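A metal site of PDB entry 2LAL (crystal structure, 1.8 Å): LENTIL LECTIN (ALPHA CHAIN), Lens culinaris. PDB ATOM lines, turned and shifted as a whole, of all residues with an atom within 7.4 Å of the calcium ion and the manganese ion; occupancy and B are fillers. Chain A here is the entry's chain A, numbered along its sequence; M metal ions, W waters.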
ATOM      1  N   ASP A  81     -28.427  30.197 -25.386  1.00  0.00           N
ATOM      2  CA  ASP A  81     -28.153  29.130 -24.414  1.00  0.00           C
ATOM      3  C   ASP A  81     -29.309  28.987 -23.432  1.00  0.00           C
ATOM      4  O   ASP A  81     -29.560  27.935 -22.844  1.00  0.00           O
ATOM      5  CB  ASP A  81     -26.867  29.450 -23.647  1.00  0.00           C
ATOM      6  CG  ASP A  81     -25.676  28.725 -24.302  1.00  0.00           C
ATOM      7  OD1 ASP A  81     -25.606  27.506 -24.136  1.00  0.00           O
ATOM      8  OD2 ASP A  81     -24.912  29.346 -25.021  1.00  0.00           O
ATOM      9  N   GLY A  82     -29.947  30.130 -23.189  1.00  0.00           N
ATOM     10  CA  GLY A  82     -31.146  30.138 -22.349  1.00  0.00           C
ATOM     11  C   GLY A  82     -31.143  31.366 -21.395  1.00  0.00           C
ATOM     12  O   GLY A  82     -30.376  32.261 -21.579  1.00  0.00           O
ATOM     13  N   GLY A  98     -22.167  31.532 -22.065  1.00  0.00           N
ATOM     14  CA  GLY A  98     -22.360  30.257 -22.834  1.00  0.00           C
ATOM     15  C   GLY A  98     -23.196  29.340 -21.967  1.00  0.00           C
ATOM     16  O   GLY A  98     -24.141  29.861 -21.393  1.00  0.00           O
ATOM     17  N   GLY A  99     -22.991  28.047 -21.877  1.00  0.00           N
ATOM     18  CA  GLY A  99     -24.024  27.225 -21.235  1.00  0.00           C
ATOM     19  C   GLY A  99     -23.936  27.461 -19.721  1.00  0.00           C
ATOM     20  O   GLY A  99     -24.737  26.806 -19.029  1.00  0.00           O
ATOM     21  N   TYR A 100     -23.008  28.249 -19.180  1.00  0.00           N
ATOM     22  CA  TYR A 100     -23.044  28.527 -17.717  1.00  0.00           C
ATOM     23  C   TYR A 100     -23.989  29.700 -17.437  1.00  0.00           C
ATOM     24  O   TYR A 100     -24.124  29.989 -16.256  1.00  0.00           O
ATOM     25  CB  TYR A 100     -21.672  28.870 -17.170  1.00  0.00           C
ATOM     26  CG  TYR A 100     -20.739  27.659 -17.052  1.00  0.00           C
ATOM     27  CD1 TYR A 100     -20.776  26.701 -16.056  1.00  0.00           C
ATOM     28  CD2 TYR A 100     -19.784  27.536 -18.059  1.00  0.00           C
ATOM     29  CE1 TYR A 100     -19.885  25.613 -16.049  1.00  0.00           C
ATOM     30  CE2 TYR A 100     -18.904  26.489 -18.040  1.00  0.00           C
ATOM     31  CZ  TYR A 100     -18.948  25.514 -17.056  1.00  0.00           C
ATOM     32  OH  TYR A 100     -17.997  24.519 -17.172  1.00  0.00           O
ATOM     33  N   LEU A 101     -24.579  30.283 -18.423  1.00  0.00           N
ATOM     34  CA  LEU A 101     -25.703  31.214 -18.459  1.00  0.00           C
ATOM     35  C   LEU A 101     -25.349  32.527 -17.736  1.00  0.00           C
ATOM     36  O   LEU A 101     -26.349  33.179 -17.343  1.00  0.00           O
ATOM     37  CB  LEU A 101     -26.968  30.617 -17.877  1.00  0.00           C
ATOM     38  CG  LEU A 101     -27.619  29.512 -18.578  1.00  0.00           C
ATOM     39  CD1 LEU A 101     -28.634  28.694 -17.803  1.00  0.00           C
ATOM     40  CD2 LEU A 101     -28.048  29.659 -20.014  1.00  0.00           C
ATOM     41  N   GLU A 119     -33.456  27.957 -14.319  1.00  0.00           N
ATOM     42  CA  GLU A 119     -33.065  28.169 -15.710  1.00  0.00           C
ATOM     43  C   GLU A 119     -34.155  27.591 -16.639  1.00  0.00           C
ATOM     44  O   GLU A 119     -34.899  26.701 -16.294  1.00  0.00           O
ATOM     45  CB  GLU A 119     -31.743  27.496 -16.027  1.00  0.00           C
ATOM     46  CG  GLU A 119     -31.904  26.038 -15.548  1.00  0.00           C
ATOM     47  CD  GLU A 119     -30.767  25.189 -15.957  1.00  0.00           C
ATOM     48  OE1 GLU A 119     -29.627  25.460 -15.696  1.00  0.00           O
ATOM     49  OE2 GLU A 119     -30.869  24.200 -16.695  1.00  0.00           O
ATOM     50  N   PHE A 120     -34.224  28.232 -17.753  1.00  0.00           N
ATOM     51  CA  PHE A 120     -35.004  27.858 -18.961  1.00  0.00           C
ATOM     52  C   PHE A 120     -33.989  27.586 -20.064  1.00  0.00           C
ATOM     53  O   PHE A 120     -33.306  28.470 -20.472  1.00  0.00           O
ATOM     54  CB  PHE A 120     -35.880  29.068 -19.336  1.00  0.00           C
ATOM     55  CG  PHE A 120     -36.772  29.353 -18.092  1.00  0.00           C
ATOM     56  CD1 PHE A 120     -37.955  28.684 -17.866  1.00  0.00           C
ATOM     57  CD2 PHE A 120     -36.333  30.302 -17.151  1.00  0.00           C
ATOM     58  CE1 PHE A 120     -38.755  28.916 -16.744  1.00  0.00           C
ATOM     59  CE2 PHE A 120     -37.089  30.569 -16.016  1.00  0.00           C
ATOM     60  CZ  PHE A 120     -38.271  29.893 -15.796  1.00  0.00           C
ATOM     61  N   ASP A 121     -33.574  26.306 -20.088  1.00  0.00           N
ATOM     62  CA  ASP A 121     -32.256  26.060 -20.739  1.00  0.00           C
ATOM     63  C   ASP A 121     -32.519  25.498 -22.148  1.00  0.00           C
ATOM     64  O   ASP A 121     -33.279  24.500 -22.179  1.00  0.00           O
ATOM     65  CB  ASP A 121     -31.485  24.999 -19.947  1.00  0.00           C
ATOM     66  CG  ASP A 121     -30.139  24.638 -20.557  1.00  0.00           C
ATOM     67  OD1 ASP A 121     -29.725  24.986 -21.675  1.00  0.00           O
ATOM     68  OD2 ASP A 121     -29.263  24.022 -19.892  1.00  0.00           O
ATOM     69  N   THR A 122     -32.072  26.078 -23.232  1.00  0.00           N
ATOM     70  CA  THR A 122     -32.501  25.822 -24.601  1.00  0.00           C
ATOM     71  C   THR A 122     -31.458  25.033 -25.388  1.00  0.00           C
ATOM     72  O   THR A 122     -31.699  24.750 -26.608  1.00  0.00           O
ATOM     73  CB  THR A 122     -32.813  27.124 -25.314  1.00  0.00           C
ATOM     74  OG1 THR A 122     -31.692  27.976 -25.319  1.00  0.00           O
ATOM     75  CG2 THR A 122     -34.001  27.783 -24.691  1.00  0.00           C
ATOM     76  N   PHE A 123     -30.372  24.607 -24.851  1.00  0.00           N
ATOM     77  CA  PHE A 123     -29.184  24.001 -25.443  1.00  0.00           C
ATOM     78  C   PHE A 123     -28.579  22.922 -24.599  1.00  0.00           C
ATOM     79  O   PHE A 123     -28.267  23.150 -23.427  1.00  0.00           O
ATOM     80  CB  PHE A 123     -28.181  25.059 -25.842  1.00  0.00           C
ATOM     81  CG  PHE A 123     -27.092  24.522 -26.748  1.00  0.00           C
ATOM     82  CD1 PHE A 123     -27.332  24.463 -28.092  1.00  0.00           C
ATOM     83  CD2 PHE A 123     -25.910  24.143 -26.112  1.00  0.00           C
ATOM     84  CE1 PHE A 123     -26.290  24.001 -28.820  1.00  0.00           C
ATOM     85  CE2 PHE A 123     -24.864  23.642 -26.887  1.00  0.00           C
ATOM     86  CZ  PHE A 123     -25.105  23.604 -28.269  1.00  0.00           C
ATOM     87  N   TYR A 124     -28.529  21.678 -25.093  1.00  0.00           N
ATOM     88  CA  TYR A 124     -27.924  20.495 -24.449  1.00  0.00           C
ATOM     89  C   TYR A 124     -26.407  20.625 -24.390  1.00  0.00           C
ATOM     90  O   TYR A 124     -25.656  20.568 -25.369  1.00  0.00           O
ATOM     91  CB  TYR A 124     -28.266  19.241 -25.264  1.00  0.00           C
ATOM     92  CG  TYR A 124     -27.653  17.971 -24.656  1.00  0.00           C
ATOM     93  CD1 TYR A 124     -28.012  17.504 -23.400  1.00  0.00           C
ATOM     94  CD2 TYR A 124     -26.709  17.221 -25.398  1.00  0.00           C
ATOM     95  CE1 TYR A 124     -27.466  16.359 -22.865  1.00  0.00           C
ATOM     96  CE2 TYR A 124     -26.141  16.067 -24.866  1.00  0.00           C
ATOM     97  CZ  TYR A 124     -26.515  15.626 -23.595  1.00  0.00           C
ATOM     98  OH  TYR A 124     -25.987  14.477 -23.043  1.00  0.00           O
ATOM     99  N   ASN A 125     -25.887  20.804 -23.191  1.00  0.00           N
ATOM    100  CA  ASN A 125     -24.469  20.695 -22.844  1.00  0.00           C
ATOM    101  C   ASN A 125     -24.212  19.305 -22.252  1.00  0.00           C
ATOM    102  O   ASN A 125     -24.816  18.999 -21.270  1.00  0.00           O
ATOM    103  CB  ASN A 125     -24.078  21.752 -21.805  1.00  0.00           C
ATOM    104  CG  ASN A 125     -24.403  23.122 -22.400  1.00  0.00           C
ATOM    105  OD1 ASN A 125     -25.559  23.730 -22.149  1.00  0.00           O
ATOM    106  ND2 ASN A 125     -23.492  23.665 -23.204  1.00  0.00           N
ATOM    107  N   ALA A 126     -23.533  18.506 -23.027  1.00  0.00           N
ATOM    108  CA  ALA A 126     -23.443  17.051 -22.824  1.00  0.00           C
ATOM    109  C   ALA A 126     -22.867  16.724 -21.449  1.00  0.00           C
ATOM    110  O   ALA A 126     -23.279  15.728 -20.846  1.00  0.00           O
ATOM    111  CB  ALA A 126     -22.469  16.504 -23.886  1.00  0.00           C
ATOM    112  N   TRP A 128     -23.325  18.148 -18.520  1.00  0.00           N
ATOM    113  CA  TRP A 128     -24.158  18.373 -17.351  1.00  0.00           C
ATOM    114  C   TRP A 128     -25.636  18.340 -17.658  1.00  0.00           C
ATOM    115  O   TRP A 128     -26.397  18.091 -16.704  1.00  0.00           O
ATOM    116  CB  TRP A 128     -23.766  19.610 -16.584  1.00  0.00           C
ATOM    117  CG  TRP A 128     -23.931  20.917 -17.352  1.00  0.00           C
ATOM    118  CD1 TRP A 128     -25.135  21.510 -17.658  1.00  0.00           C
ATOM    119  CD2 TRP A 128     -22.897  21.728 -17.879  1.00  0.00           C
ATOM    120  NE1 TRP A 128     -24.828  22.691 -18.392  1.00  0.00           N
ATOM    121  CE2 TRP A 128     -23.528  22.815 -18.527  1.00  0.00           C
ATOM    122  CE3 TRP A 128     -21.513  21.698 -17.890  1.00  0.00           C
ATOM    123  CZ2 TRP A 128     -22.816  23.766 -19.108  1.00  0.00           C
ATOM    124  CZ3 TRP A 128     -20.774  22.678 -18.514  1.00  0.00           C
ATOM    125  CH2 TRP A 128     -21.427  23.715 -19.126  1.00  0.00           C
ATOM    126  N   ASP A 129     -26.142  18.600 -18.844  1.00  0.00           N
ATOM    127  CA  ASP A 129     -27.589  18.668 -19.106  1.00  0.00           C
ATOM    128  C   ASP A 129     -28.191  17.274 -19.125  1.00  0.00           C
ATOM    129  O   ASP A 129     -27.407  16.350 -19.375  1.00  0.00           O
ATOM    130  CB  ASP A 129     -27.852  19.354 -20.449  1.00  0.00           C
ATOM    131  CG  ASP A 129     -27.774  20.857 -20.141  1.00  0.00           C
ATOM    132  OD1 ASP A 129     -28.018  21.174 -18.933  1.00  0.00           O
ATOM    133  OD2 ASP A 129     -27.515  21.680 -20.969  1.00  0.00           O
ATOM    134  N   PRO A 130     -29.500  17.138 -18.860  1.00  0.00           N
ATOM    135  CA  PRO A 130     -30.135  15.807 -18.909  1.00  0.00           C
ATOM    136  C   PRO A 130     -29.958  15.190 -20.292  1.00  0.00           C
ATOM    137  O   PRO A 130     -29.987  15.846 -21.327  1.00  0.00           O
ATOM    138  CB  PRO A 130     -31.580  16.168 -18.672  1.00  0.00           C
ATOM    139  CG  PRO A 130     -31.655  17.541 -18.099  1.00  0.00           C
ATOM    140  CD  PRO A 130     -30.486  18.242 -18.705  1.00  0.00           C
ATOM    141  N   GLU A 134     -33.379  17.019 -24.078  1.00  0.00           N
ATOM    142  CA  GLU A 134     -34.351  18.057 -24.371  1.00  0.00           C
ATOM    143  C   GLU A 134     -34.133  19.304 -23.554  1.00  0.00           C
ATOM    144  O   GLU A 134     -33.330  19.363 -22.654  1.00  0.00           O
ATOM    145  CB  GLU A 134     -35.764  17.591 -24.374  1.00  0.00           C
ATOM    146  CG  GLU A 134     -36.137  16.493 -23.502  1.00  0.00           C
ATOM    147  CD  GLU A 134     -37.302  15.667 -24.009  1.00  0.00           C
ATOM    148  OE1 GLU A 134     -37.239  15.210 -25.154  1.00  0.00           O
ATOM    149  OE2 GLU A 134     -38.299  15.404 -23.316  1.00  0.00           O
ATOM    150  N   HIS A 136     -35.346  22.434 -21.134  1.00  0.00           N
ATOM    151  CA  HIS A 136     -35.860  22.065 -19.816  1.00  0.00           C
ATOM    152  C   HIS A 136     -35.778  23.270 -18.870  1.00  0.00           C
ATOM    153  O   HIS A 136     -35.030  24.186 -19.139  1.00  0.00           O
ATOM    154  CB  HIS A 136     -35.122  20.867 -19.223  1.00  0.00           C
ATOM    155  CG  HIS A 136     -33.604  21.060 -19.248  1.00  0.00           C
ATOM    156  ND1 HIS A 136     -32.756  20.960 -20.358  1.00  0.00           N
ATOM    157  CD2 HIS A 136     -32.818  21.403 -18.125  1.00  0.00           C
ATOM    158  CE1 HIS A 136     -31.477  21.263 -19.946  1.00  0.00           C
ATOM    159  NE2 HIS A 136     -31.514  21.559 -18.592  1.00  0.00           N
ATOM    160  N   ILE A 137     -36.652  23.231 -17.911  1.00  0.00           N
ATOM    161  CA  ILE A 137     -36.651  24.084 -16.712  1.00  0.00           C
ATOM    162  C   ILE A 137     -35.761  23.453 -15.640  1.00  0.00           C
ATOM    163  O   ILE A 137     -35.932  22.227 -15.550  1.00  0.00           O
ATOM    164  CB  ILE A 137     -38.092  24.186 -16.177  1.00  0.00           C
ATOM    165  CG1 ILE A 137     -39.004  24.737 -17.268  1.00  0.00           C
ATOM    166  CG2 ILE A 137     -38.157  25.008 -14.910  1.00  0.00           C
ATOM    167  CD1 ILE A 137     -40.415  24.249 -17.305  1.00  0.00           C
ATOM    168  N   GLY A 138     -34.860  24.105 -14.985  1.00  0.00           N
ATOM    169  CA  GLY A 138     -34.087  23.455 -13.882  1.00  0.00           C
ATOM    170  C   GLY A 138     -34.064  24.360 -12.648  1.00  0.00           C
ATOM    171  O   GLY A 138     -34.174  25.599 -12.767  1.00  0.00           O
ATOM    172  N   ASP A 140     -31.226  25.257  -9.981  1.00  0.00           N
ATOM    173  CA  ASP A 140     -29.767  25.270  -9.834  1.00  0.00           C
ATOM    174  C   ASP A 140     -29.343  25.854  -8.498  1.00  0.00           C
ATOM    175  O   ASP A 140     -29.701  26.987  -8.169  1.00  0.00           O
ATOM    176  CB  ASP A 140     -29.128  26.073 -10.967  1.00  0.00           C
ATOM    177  CG  ASP A 140     -29.546  25.555 -12.346  1.00  0.00           C
ATOM    178  OD1 ASP A 140     -30.132  24.507 -12.502  1.00  0.00           O
ATOM    179  OD2 ASP A 140     -29.198  26.283 -13.249  1.00  0.00           O
ATOM    180  N   ILE A 144     -24.219  24.684 -12.277  1.00  0.00           N
ATOM    181  CA  ILE A 144     -24.915  24.597 -13.561  1.00  0.00           C
ATOM    182  C   ILE A 144     -25.627  23.295 -13.788  1.00  0.00           C
ATOM    183  O   ILE A 144     -26.572  23.105 -14.553  1.00  0.00           O
ATOM    184  CB  ILE A 144     -24.017  24.959 -14.721  1.00  0.00           C
ATOM    185  CG1 ILE A 144     -24.795  25.419 -15.930  1.00  0.00           C
ATOM    186  CG2 ILE A 144     -23.061  23.824 -15.069  1.00  0.00           C
ATOM    187  CD1 ILE A 144     -25.714  26.608 -15.798  1.00  0.00           C
ATOM    188  N   LYS A 145     -25.239  22.276 -13.014  1.00  0.00           N
ATOM    189  CA  LYS A 145     -25.977  20.995 -13.090  1.00  0.00           C
ATOM    190  C   LYS A 145     -27.214  21.061 -12.184  1.00  0.00           C
ATOM    191  O   LYS A 145     -26.957  21.024 -10.970  1.00  0.00           O
ATOM    192  CB  LYS A 145     -25.057  19.911 -12.472  1.00  0.00           C
ATOM    193  CG  LYS A 145     -24.793  18.860 -13.546  1.00  0.00           C
ATOM    194  CD  LYS A 145     -25.448  17.566 -13.102  1.00  0.00           C
ATOM    195  CE  LYS A 145     -24.906  17.250 -11.716  1.00  0.00           C
ATOM    196  NZ  LYS A 145     -25.719  16.190 -11.106  1.00  0.00           N
ATOM    197  N   SER A 146     -28.416  21.138 -12.686  1.00  0.00           N
ATOM    198  CA  SER A 146     -29.647  21.362 -11.923  1.00  0.00           C
ATOM    199  C   SER A 146     -29.849  20.322 -10.849  1.00  0.00           C
ATOM    200  O   SER A 146     -29.496  19.148 -11.088  1.00  0.00           O
ATOM    201  CB  SER A 146     -30.846  21.423 -12.853  1.00  0.00           C
ATOM    202  OG  SER A 146     -30.476  22.268 -13.940  1.00  0.00           O
ATOM    203  N   THR A 149     -34.941  18.946 -12.923  1.00  0.00           N
ATOM    204  CA  THR A 149     -35.261  19.423 -14.271  1.00  0.00           C
ATOM    205  C   THR A 149     -36.627  18.902 -14.697  1.00  0.00           C
ATOM    206  O   THR A 149     -37.089  17.873 -14.213  1.00  0.00           O
ATOM    207  CB  THR A 149     -34.205  19.094 -15.275  1.00  0.00           C
ATOM    208  OG1 THR A 149     -34.106  17.689 -15.542  1.00  0.00           O
ATOM    209  CG2 THR A 149     -32.862  19.585 -14.851  1.00  0.00           C
HETATM  210 CA    CA M   1     -27.680  23.986 -21.445  1.00  0.00          CA
HETATM  211 MN    MN M   2     -29.526  22.677 -17.928  1.00  0.00          MN
HETATM  212  O   HOH W   1     -26.578  24.917 -19.558  1.00  0.00           O
HETATM  213  O   HOH W   2     -29.646  21.347 -16.241  1.00  0.00           O
HETATM  214  O   HOH W   3     -27.464  26.146 -22.458  1.00  0.00           O
HETATM  215  O   HOH W   4     -27.919  23.751 -16.876  1.00  0.00           O
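O of Glu 134 is in hydrogen-bond range of ND1 of His 136. OE2 of Glu 119 sits close to OG of Ser 146, at 3.4 Å. The side-chain carboxylate (OD2) of Asp 140 sits close to the side-chain carboxylate (OE1) of Glu 119, 2.6 Å away. The backbone NH of Gly 138 is in hydrogen-bond range of the backbone carbonyl oxygen of Glu 119, at 2.9 Å.
Of the 26 residues printed, 4 come within 4 Å of the calcium ion. The nearest printed residue that does not touch the calcium ion is Trp 128 (4.4 Å).
Four residues have an atom within 4 Å of the manganese ion: Glu 119, Asp 121, Asp 129 and His 136. Along chain A the residues within 4 Å of the manganese ion span positions 119 to 136. The nearest printed residue that does not touch the manganese ion is Ser 146 (4.1 Å).
The calcium ion is bound by OD2 of Asp 121 (2.2 Å). The calcium ion is bound by the backbone carbonyl oxygen (O) of Phe 123, 2.2 Å away. The calcium ion is bound by the side-chain amide oxygen (OD1) of Asn 125, at 2.2 Å. The side-chain carboxylate (OD1) of Asp 121 is bound to the calcium ion (2.3 Å). OD2 of Asp 129 is bound to the calcium ion, 2.4 Å away. Water W1 binds the calcium ion (2.4 Å). The calcium ion is bound by water W3 (2.4 Å).
Water W2 is bound to the manganese ion (2.2 Å). Water W4 binds the manganese ion. The manganese ion is bound by OD1 of Asp 129, 2.4 Å away. NE2 of His 136 binds the manganese ion, 2.4 Å away. OE2 of Glu 119 binds the manganese ion (2.4 Å). The manganese ion is bound by OD2 of Asp 121 (2.4 Å).
Water W1 lies within hydrogen-bond range of the backbone carbonyl oxygen of Gly 99 (2.7 Å) and the indole nitrogen of Trp 128 (3.1 Å). Water W4 bridges OE1 of Glu 119 (2.7 Å) and O of Ile 144 (2.8 Å).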
